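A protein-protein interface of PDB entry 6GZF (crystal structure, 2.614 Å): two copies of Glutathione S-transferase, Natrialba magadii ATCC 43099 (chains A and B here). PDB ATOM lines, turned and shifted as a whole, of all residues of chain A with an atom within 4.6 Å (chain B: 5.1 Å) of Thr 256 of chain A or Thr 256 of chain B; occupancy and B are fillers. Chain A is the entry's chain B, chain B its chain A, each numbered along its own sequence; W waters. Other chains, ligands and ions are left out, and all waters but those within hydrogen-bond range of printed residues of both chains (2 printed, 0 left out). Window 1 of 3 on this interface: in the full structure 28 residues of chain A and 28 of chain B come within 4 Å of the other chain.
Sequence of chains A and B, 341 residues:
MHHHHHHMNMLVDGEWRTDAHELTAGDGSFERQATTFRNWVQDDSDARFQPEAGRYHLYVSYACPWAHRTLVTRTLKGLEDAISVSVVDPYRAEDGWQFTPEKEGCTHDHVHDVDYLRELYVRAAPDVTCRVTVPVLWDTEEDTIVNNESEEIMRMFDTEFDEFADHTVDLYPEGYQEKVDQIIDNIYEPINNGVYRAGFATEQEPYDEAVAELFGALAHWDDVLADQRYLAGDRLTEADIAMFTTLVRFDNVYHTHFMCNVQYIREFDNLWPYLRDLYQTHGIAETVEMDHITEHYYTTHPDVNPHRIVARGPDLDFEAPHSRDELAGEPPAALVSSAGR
The backbone carbonyl oxygen of His 255 of chain B lies within hydrogen-bond range of the backbone NH of Cys 260 of chain B (3.2 Å).
The backbone carbonyl oxygen (O) of Met 259 of chain A sits close to the side-chain amide oxygen (OD1) of Asn 261 of chain A (3.3 Å).
N of His 255 of chain B is in hydrogen-bond range of O of Phe 250 of chain B.
The backbone NH (N) of Met 259 of chain B sits at hydrogen-bond distance from the backbone carbonyl oxygen (O) of Tyr 254 of chain B (3.3 Å).
The backbone carbonyl oxygen of Tyr 254 of chain A lies within hydrogen-bond range of the backbone NH of Met 259 of chain A (3.5 Å).
The side-chain amide oxygen of Asn 261 of chain B sits close to the backbone carbonyl oxygen of Met 259 of chain B, at 3.4 Å.
His 255 of chain B touches its own counterpart, His 255 of chain A.
Thr 256 of chain B touches its own counterpart, Thr 256 of chain A.
Thr 256 of chain A touches Met 259 of chain B, and with the chains exchanged Met 259 of chain A touches Thr 256 of chain B.
Thr 256 of chain A touches Asn 261 of chain B, and with the chains exchanged Asn 261 of chain A touches Thr 256 of chain B.
Positions printed for both chains: 253, 254, 255, 256, 257, 258, 259, 261 and 298.
Of the 12 pairs that touch across the chains among the printed residues, 10 have their exchanged pair printed and touching as well.
Water W2 lies within hydrogen-bond range of OG1 of Thr 256 of chain B (2.6 Å), ND1 of His 255 of chain B (2.7 Å), OG1 of Thr 256 of chain A (2.8 Å) and ND1 of His 255 of chain A (2.8 Å).
Water W1 lies within hydrogen-bond range of OG1 of Thr 256 of chain B (2.8 Å) and ND2 of Asn 261 of chain A (3.0 Å).
CE1 of His 255 of chain A touches CE1 of His 255 of chain B, 3.5 Å away.
Thr 256 of chain A touches Thr 256 of chain B.
Thr 256 of chain A touches Met 259 of chain B.
CG of Met 259 of chain A touches CG2 of Thr 256 of chain B, at 3.7 Å.
Met 259 of chain A touches Tyr 298 of chain B.
CB of Ala 311 of chain B touches SD of Met 259 of chain A, 3.9 Å away.
Tyr 298 of chain B touches Asn 261 of chain A (OH to ND2, 3.97 Å).
OD1 of Asn 261 of chain A touches CB of Ala 311 of chain B, at 3.9 Å.
Met 259 of chain B touches Tyr 298 of chain A.
OH of Tyr 298 of chain A touches ND2 of Asn 261 of chain B, 3.97 Å away.
Hydrophobic or aromatic side chains of chain A within 4 Å of the printed part of chain B: His 255, Met 259 and Tyr 298.
Along chain A the printed residues that touch a printed residue of chain B span positions 255 to 298.
Of the 12 printed residues of chain B, 6 touch a printed residue of chain A.
Printed residues of chain B that touch a printed residue of chain A: His 255, Thr 256, Met 259, Asn 261, Tyr 298 and Ala 311.
Among the printed residues, no Asp or Glu carboxylate lies within 4 Å of a Lys or Arg side-chain nitrogen of the other chain.
ND2 of Asn 261 of chain B is in hydrogen-bond range of OG1 of Thr 256 of chain A, at 2.8 Å.
The side-chain amide nitrogen (ND2) of Asn 261 of chain A lies within hydrogen-bond range of the side-chain hydroxyl (OG1) of Thr 256 of chain B.
Thr 256 of chain A touches just these residues of chain B: Thr 256, Met 259 and Asn 261.
Thr 256 of chain B touches three residues of chain A.
Of the printed residues of chain A, Met 259 of chain B touches Thr 256 and Tyr 298.
Printed residues of chain A within 4 Å of Asn 261 of chain B: Thr 256 (2.8 Å) and Tyr 298 (3.97 Å).
Of the printed residues of chain A, Tyr 298 of chain B touches Met 259 and Asn 261.
The nearest residue of chain B that does not touch Thr 256 of chain A is His 255 of chain B (4.1 Å).
The nearest residue of chain A that does not touch Thr 256 of chain B is His 255 of chain A (4.3 Å).
The nearest printed residue of chain A that does not touch Met 259 of chain B is His 257 of chain A (5.8 Å).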
ATOM      1  N   VAL A 253       7.635  14.859   4.709  1.00  0.00           N
ATOM      2  CA  VAL A 253       8.006  14.520   6.081  1.00  0.00           C
ATOM      3  C   VAL A 253       9.373  13.842   6.197  1.00  0.00           C
ATOM      4  O   VAL A 253      10.298  14.410   6.776  1.00  0.00           O
ATOM      5  CB  VAL A 253       6.949  13.603   6.734  1.00  0.00           C
ATOM      6  CG1 VAL A 253       7.405  13.169   8.118  1.00  0.00           C
ATOM      7  CG2 VAL A 253       5.603  14.306   6.810  1.00  0.00           C
ATOM      8  N   TYR A 254       9.488  12.632   5.651  1.00  0.00           N
ATOM      9  CA  TYR A 254      10.687  11.804   5.814  1.00  0.00           C
ATOM     10  C   TYR A 254      11.973  12.527   5.425  1.00  0.00           C
ATOM     11  O   TYR A 254      12.990  12.417   6.111  1.00  0.00           O
ATOM     12  CB  TYR A 254      10.563  10.521   4.988  1.00  0.00           C
ATOM     13  CG  TYR A 254       9.439   9.605   5.414  1.00  0.00           C
ATOM     14  CD1 TYR A 254       9.017   9.557   6.736  1.00  0.00           C
ATOM     15  CD2 TYR A 254       8.804   8.783   4.492  1.00  0.00           C
ATOM     16  CE1 TYR A 254       7.990   8.717   7.127  1.00  0.00           C
ATOM     17  CE2 TYR A 254       7.777   7.941   4.874  1.00  0.00           C
ATOM     18  CZ  TYR A 254       7.374   7.911   6.191  1.00  0.00           C
ATOM     19  OH  TYR A 254       6.352   7.071   6.569  1.00  0.00           O
ATOM     20  N   HIS A 255      11.917  13.261   4.319  1.00  0.00           N
ATOM     21  CA  HIS A 255      13.072  13.983   3.801  1.00  0.00           C
ATOM     22  C   HIS A 255      13.599  15.008   4.802  1.00  0.00           C
ATOM     23  O   HIS A 255      14.794  15.053   5.092  1.00  0.00           O
ATOM     24  CB  HIS A 255      12.708  14.673   2.483  1.00  0.00           C
ATOM     25  CG  HIS A 255      13.861  15.349   1.810  1.00  0.00           C
ATOM     26  ND1 HIS A 255      14.353  16.569   2.220  1.00  0.00           N
ATOM     27  CD2 HIS A 255      14.613  14.978   0.746  1.00  0.00           C
ATOM     28  CE1 HIS A 255      15.360  16.919   1.441  1.00  0.00           C
ATOM     29  NE2 HIS A 255      15.539  15.972   0.539  1.00  0.00           N
ATOM     30  N   THR A 256      12.694  15.823   5.334  1.00  0.00           N
ATOM     31  CA  THR A 256      13.074  16.903   6.236  1.00  0.00           C
ATOM     32  C   THR A 256      13.041  16.486   7.703  1.00  0.00           C
ATOM     33  O   THR A 256      14.057  16.549   8.397  1.00  0.00           O
ATOM     34  CB  THR A 256      12.155  18.121   6.054  1.00  0.00           C
ATOM     35  OG1 THR A 256      12.196  18.552   4.689  1.00  0.00           O
ATOM     36  CG2 THR A 256      12.605  19.256   6.952  1.00  0.00           C
ATOM     37  N   HIS A 257      11.868  16.067   8.167  1.00  0.00           N
ATOM     38  CA  HIS A 257      11.656  15.737   9.573  1.00  0.00           C
ATOM     39  C   HIS A 257      12.565  14.609  10.057  1.00  0.00           C
ATOM     40  O   HIS A 257      13.136  14.690  11.146  1.00  0.00           O
ATOM     41  CB  HIS A 257      10.192  15.362   9.809  1.00  0.00           C
ATOM     42  CG  HIS A 257       9.868  15.060  11.238  1.00  0.00           C
ATOM     43  ND1 HIS A 257      10.031  15.981  12.250  1.00  0.00           N
ATOM     44  CD2 HIS A 257       9.386  13.938  11.825  1.00  0.00           C
ATOM     45  CE1 HIS A 257       9.666  15.440  13.399  1.00  0.00           C
ATOM     46  NE2 HIS A 257       9.271  14.200  13.168  1.00  0.00           N
ATOM     47  N   PHE A 258      12.698  13.563   9.249  1.00  0.00           N
ATOM     48  CA  PHE A 258      13.542  12.428   9.609  1.00  0.00           C
ATOM     49  C   PHE A 258      14.937  12.550   9.006  1.00  0.00           C
ATOM     50  O   PHE A 258      15.729  11.607   9.059  1.00  0.00           O
ATOM     51  CB  PHE A 258      12.892  11.114   9.170  1.00  0.00           C
ATOM     52  CG  PHE A 258      11.806  10.637  10.093  1.00  0.00           C
ATOM     53  CD1 PHE A 258      11.657  11.190  11.354  1.00  0.00           C
ATOM     54  CD2 PHE A 258      10.939   9.631   9.703  1.00  0.00           C
ATOM     55  CE1 PHE A 258      10.663  10.751  12.206  1.00  0.00           C
ATOM     56  CE2 PHE A 258       9.942   9.189  10.551  1.00  0.00           C
ATOM     57  CZ  PHE A 258       9.804   9.751  11.804  1.00  0.00           C
ATOM     58  N   MET A 259      15.221  13.716   8.430  1.00  0.00           N
ATOM     59  CA  MET A 259      16.535  14.032   7.870  1.00  0.00           C
ATOM     60  C   MET A 259      17.023  13.026   6.829  1.00  0.00           C
ATOM     61  O   MET A 259      18.217  12.744   6.740  1.00  0.00           O
ATOM     62  CB  MET A 259      17.572  14.150   8.989  1.00  0.00           C
ATOM     63  CG  MET A 259      17.411  15.383   9.861  1.00  0.00           C
ATOM     64  SD  MET A 259      18.778  15.584  11.019  1.00  0.00           S
ATOM     65  CE  MET A 259      18.427  17.210  11.682  1.00  0.00           C
ATOM     66  N   ASN A 261      17.581  13.411   3.693  1.00  0.00           N
ATOM     67  CA  ASN A 261      17.646  14.527   2.756  1.00  0.00           C
ATOM     68  C   ASN A 261      18.714  14.414   1.671  1.00  0.00           C
ATOM     69  O   ASN A 261      19.300  15.419   1.270  1.00  0.00           O
ATOM     70  CB  ASN A 261      17.868  15.823   3.534  1.00  0.00           C
ATOM     71  CG  ASN A 261      19.163  15.812   4.326  1.00  0.00           C
ATOM     72  OD1 ASN A 261      19.708  14.752   4.631  1.00  0.00           O
ATOM     73  ND2 ASN A 261      19.661  16.997   4.664  1.00  0.00           N
ATOM     74  N   TYR A 298       5.225  16.282  12.852  1.00  0.00           N
ATOM     75  CA  TYR A 298       5.861  17.522  13.285  1.00  0.00           C
ATOM     76  C   TYR A 298       5.396  17.990  14.664  1.00  0.00           C
ATOM     77  O   TYR A 298       5.966  18.924  15.222  1.00  0.00           O
ATOM     78  CB  TYR A 298       5.615  18.632  12.259  1.00  0.00           C
ATOM     79  CG  TYR A 298       6.426  18.488  10.989  1.00  0.00           C
ATOM     80  CD1 TYR A 298       7.799  18.693  10.994  1.00  0.00           C
ATOM     81  CD2 TYR A 298       5.817  18.158   9.785  1.00  0.00           C
ATOM     82  CE1 TYR A 298       8.546  18.566   9.837  1.00  0.00           C
ATOM     83  CE2 TYR A 298       6.556  18.028   8.622  1.00  0.00           C
ATOM     84  CZ  TYR A 298       7.919  18.233   8.655  1.00  0.00           C
ATOM     85  OH  TYR A 298       8.656  18.107   7.500  1.00  0.00           O
ATOM     86  N   PHE B 250      22.456  26.311   1.968  1.00  0.00           N
ATOM     87  CA  PHE B 250      21.014  26.088   1.929  1.00  0.00           C
ATOM     88  C   PHE B 250      20.631  24.611   1.856  1.00  0.00           C
ATOM     89  O   PHE B 250      19.835  24.134   2.663  1.00  0.00           O
ATOM     90  CB  PHE B 250      20.401  26.838   0.745  1.00  0.00           C
ATOM     91  CG  PHE B 250      18.922  27.089   0.881  1.00  0.00           C
ATOM     92  CD1 PHE B 250      18.004  26.086   0.617  1.00  0.00           C
ATOM     93  CD2 PHE B 250      18.452  28.331   1.269  1.00  0.00           C
ATOM     94  CE1 PHE B 250      16.648  26.318   0.743  1.00  0.00           C
ATOM     95  CE2 PHE B 250      17.097  28.568   1.395  1.00  0.00           C
ATOM     96  CZ  PHE B 250      16.194  27.561   1.133  1.00  0.00           C
ATOM     97  N   VAL B 253      22.089  22.432   4.926  1.00  0.00           N
ATOM     98  CA  VAL B 253      21.709  22.825   6.279  1.00  0.00           C
ATOM     99  C   VAL B 253      20.321  23.461   6.360  1.00  0.00           C
ATOM    100  O   VAL B 253      19.412  22.901   6.973  1.00  0.00           O
ATOM    101  CB  VAL B 253      22.731  23.812   6.876  1.00  0.00           C
ATOM    102  CG1 VAL B 253      22.234  24.351   8.206  1.00  0.00           C
ATOM    103  CG2 VAL B 253      24.087  23.144   7.040  1.00  0.00           C
ATOM    104  N   TYR B 254      20.169  24.629   5.742  1.00  0.00           N
ATOM    105  CA  TYR B 254      18.955  25.435   5.871  1.00  0.00           C
ATOM    106  C   TYR B 254      17.688  24.681   5.474  1.00  0.00           C
ATOM    107  O   TYR B 254      16.648  24.813   6.119  1.00  0.00           O
ATOM    108  CB  TYR B 254      19.080  26.704   5.025  1.00  0.00           C
ATOM    109  CG  TYR B 254      20.161  27.655   5.489  1.00  0.00           C
ATOM    110  CD1 TYR B 254      20.577  27.674   6.814  1.00  0.00           C
ATOM    111  CD2 TYR B 254      20.770  28.529   4.598  1.00  0.00           C
ATOM    112  CE1 TYR B 254      21.566  28.543   7.240  1.00  0.00           C
ATOM    113  CE2 TYR B 254      21.759  29.399   5.015  1.00  0.00           C
ATOM    114  CZ  TYR B 254      22.152  29.402   6.336  1.00  0.00           C
ATOM    115  OH  TYR B 254      23.136  30.268   6.754  1.00  0.00           O
ATOM    116  N   HIS B 255      17.792  23.889   4.413  1.00  0.00           N
ATOM    117  CA  HIS B 255      16.657  23.153   3.868  1.00  0.00           C
ATOM    118  C   HIS B 255      16.088  22.140   4.861  1.00  0.00           C
ATOM    119  O   HIS B 255      14.871  22.010   4.999  1.00  0.00           O
ATOM    120  CB  HIS B 255      17.077  22.446   2.577  1.00  0.00           C
ATOM    121  CG  HIS B 255      15.947  21.800   1.839  1.00  0.00           C
ATOM    122  ND1 HIS B 255      15.325  20.653   2.283  1.00  0.00           N
ATOM    123  CD2 HIS B 255      15.333  22.135   0.680  1.00  0.00           C
ATOM    124  CE1 HIS B 255      14.375  20.311   1.432  1.00  0.00           C
ATOM    125  NE2 HIS B 255      14.358  21.196   0.450  1.00  0.00           N
ATOM    126  N   THR B 256      16.972  21.431   5.554  1.00  0.00           N
ATOM    127  CA  THR B 256      16.557  20.366   6.461  1.00  0.00           C
ATOM    128  C   THR B 256      16.579  20.799   7.922  1.00  0.00           C
ATOM    129  O   THR B 256      15.569  20.704   8.622  1.00  0.00           O
ATOM    130  CB  THR B 256      17.452  19.125   6.305  1.00  0.00           C
ATOM    131  OG1 THR B 256      17.296  18.587   4.988  1.00  0.00           O
ATOM    132  CG2 THR B 256      17.076  18.066   7.328  1.00  0.00           C
ATOM    133  N   HIS B 257      17.737  21.268   8.374  1.00  0.00           N
ATOM    134  CA  HIS B 257      17.925  21.646   9.771  1.00  0.00           C
ATOM    135  C   HIS B 257      17.021  22.806  10.179  1.00  0.00           C
ATOM    136  O   HIS B 257      16.459  22.809  11.274  1.00  0.00           O
ATOM    137  CB  HIS B 257      19.389  22.008  10.030  1.00  0.00           C
ATOM    138  CG  HIS B 257      19.675  22.391  11.447  1.00  0.00           C
ATOM    139  ND1 HIS B 257      19.400  21.560  12.513  1.00  0.00           N
ATOM    140  CD2 HIS B 257      20.213  23.515  11.978  1.00  0.00           C
ATOM    141  CE1 HIS B 257      19.754  22.155  13.636  1.00  0.00           C
ATOM    142  NE2 HIS B 257      20.252  23.343  13.340  1.00  0.00           N
ATOM    143  N   PHE B 258      16.883  23.789   9.295  1.00  0.00           N
ATOM    144  CA  PHE B 258      16.036  24.945   9.568  1.00  0.00           C
ATOM    145  C   PHE B 258      14.663  24.802   8.916  1.00  0.00           C
ATOM    146  O   PHE B 258      13.852  25.727   8.951  1.00  0.00           O
ATOM    147  CB  PHE B 258      16.713  26.233   9.089  1.00  0.00           C
ATOM    148  CG  PHE B 258      17.722  26.783  10.057  1.00  0.00           C
ATOM    149  CD1 PHE B 258      17.872  26.224  11.315  1.00  0.00           C
ATOM    150  CD2 PHE B 258      18.516  27.864   9.713  1.00  0.00           C
ATOM    151  CE1 PHE B 258      18.796  26.731  12.208  1.00  0.00           C
ATOM    152  CE2 PHE B 258      19.442  28.373  10.601  1.00  0.00           C
ATOM    153  CZ  PHE B 258      19.582  27.806  11.850  1.00  0.00           C
ATOM    154  N   MET B 259      14.424  23.637   8.317  1.00  0.00           N
ATOM    155  CA  MET B 259      13.126  23.291   7.740  1.00  0.00           C
ATOM    156  C   MET B 259      12.647  24.268   6.665  1.00  0.00           C
ATOM    157  O   MET B 259      11.448  24.513   6.532  1.00  0.00           O
ATOM    158  CB  MET B 259      12.073  23.180   8.847  1.00  0.00           C
ATOM    159  CG  MET B 259      11.832  21.757   9.323  1.00  0.00           C
ATOM    160  SD  MET B 259      10.849  21.652  10.829  1.00  0.00           S
ATOM    161  CE  MET B 259      12.133  21.748  12.073  1.00  0.00           C
ATOM    162  N   CYS B 260      13.583  24.821   5.901  1.00  0.00           N
ATOM    163  CA  CYS B 260      13.235  25.622   4.733  1.00  0.00           C
ATOM    164  C   CYS B 260      13.132  24.702   3.523  1.00  0.00           C
ATOM    165  O   CYS B 260      13.957  24.759   2.613  1.00  0.00           O
ATOM    166  CB  CYS B 260      14.275  26.719   4.494  1.00  0.00           C
ATOM    167  SG  CYS B 260      14.464  27.876   5.871  1.00  0.00           S
ATOM    168  N   ASN B 261      12.106  23.856   3.517  1.00  0.00           N
ATOM    169  CA  ASN B 261      12.053  22.724   2.597  1.00  0.00           C
ATOM    170  C   ASN B 261      11.022  22.826   1.474  1.00  0.00           C
ATOM    171  O   ASN B 261      10.401  21.828   1.109  1.00  0.00           O
ATOM    172  CB  ASN B 261      11.790  21.443   3.393  1.00  0.00           C
ATOM    173  CG  ASN B 261      10.436  21.450   4.080  1.00  0.00           C
ATOM    174  OD1 ASN B 261       9.835  22.506   4.285  1.00  0.00           O
ATOM    175  ND2 ASN B 261       9.947  20.266   4.435  1.00  0.00           N
ATOM    176  N   TYR B 298      24.350  21.305  13.032  1.00  0.00           N
ATOM    177  CA  TYR B 298      23.653  20.088  13.442  1.00  0.00           C
ATOM    178  C   TYR B 298      23.963  19.641  14.874  1.00  0.00           C
ATOM    179  O   TYR B 298      23.216  18.846  15.442  1.00  0.00           O
ATOM    180  CB  TYR B 298      23.964  18.945  12.470  1.00  0.00           C
ATOM    181  CG  TYR B 298      23.207  19.036  11.160  1.00  0.00           C
ATOM    182  CD1 TYR B 298      21.858  18.709  11.092  1.00  0.00           C
ATOM    183  CD2 TYR B 298      23.842  19.441   9.992  1.00  0.00           C
ATOM    184  CE1 TYR B 298      21.161  18.791   9.901  1.00  0.00           C
ATOM    185  CE2 TYR B 298      23.152  19.525   8.796  1.00  0.00           C
ATOM    186  CZ  TYR B 298      21.813  19.198   8.756  1.00  0.00           C
ATOM    187  OH  TYR B 298      21.121  19.279   7.569  1.00  0.00           O
ATOM    188  N   ALA B 311      23.172  15.441   9.623  1.00  0.00           N
ATOM    189  CA  ALA B 311      22.489  14.895   8.458  1.00  0.00           C
ATOM    190  C   ALA B 311      23.449  14.770   7.281  1.00  0.00           C
ATOM    191  O   ALA B 311      24.400  15.542   7.158  1.00  0.00           O
ATOM    192  CB  ALA B 311      21.296  15.760   8.084  1.00  0.00           C
HETATM  193  O   HOH W   1      19.456  19.846   3.842  1.00  0.00           O
HETATM  194  O   HOH W   2      14.896  18.661   4.069  1.00  0.00           O
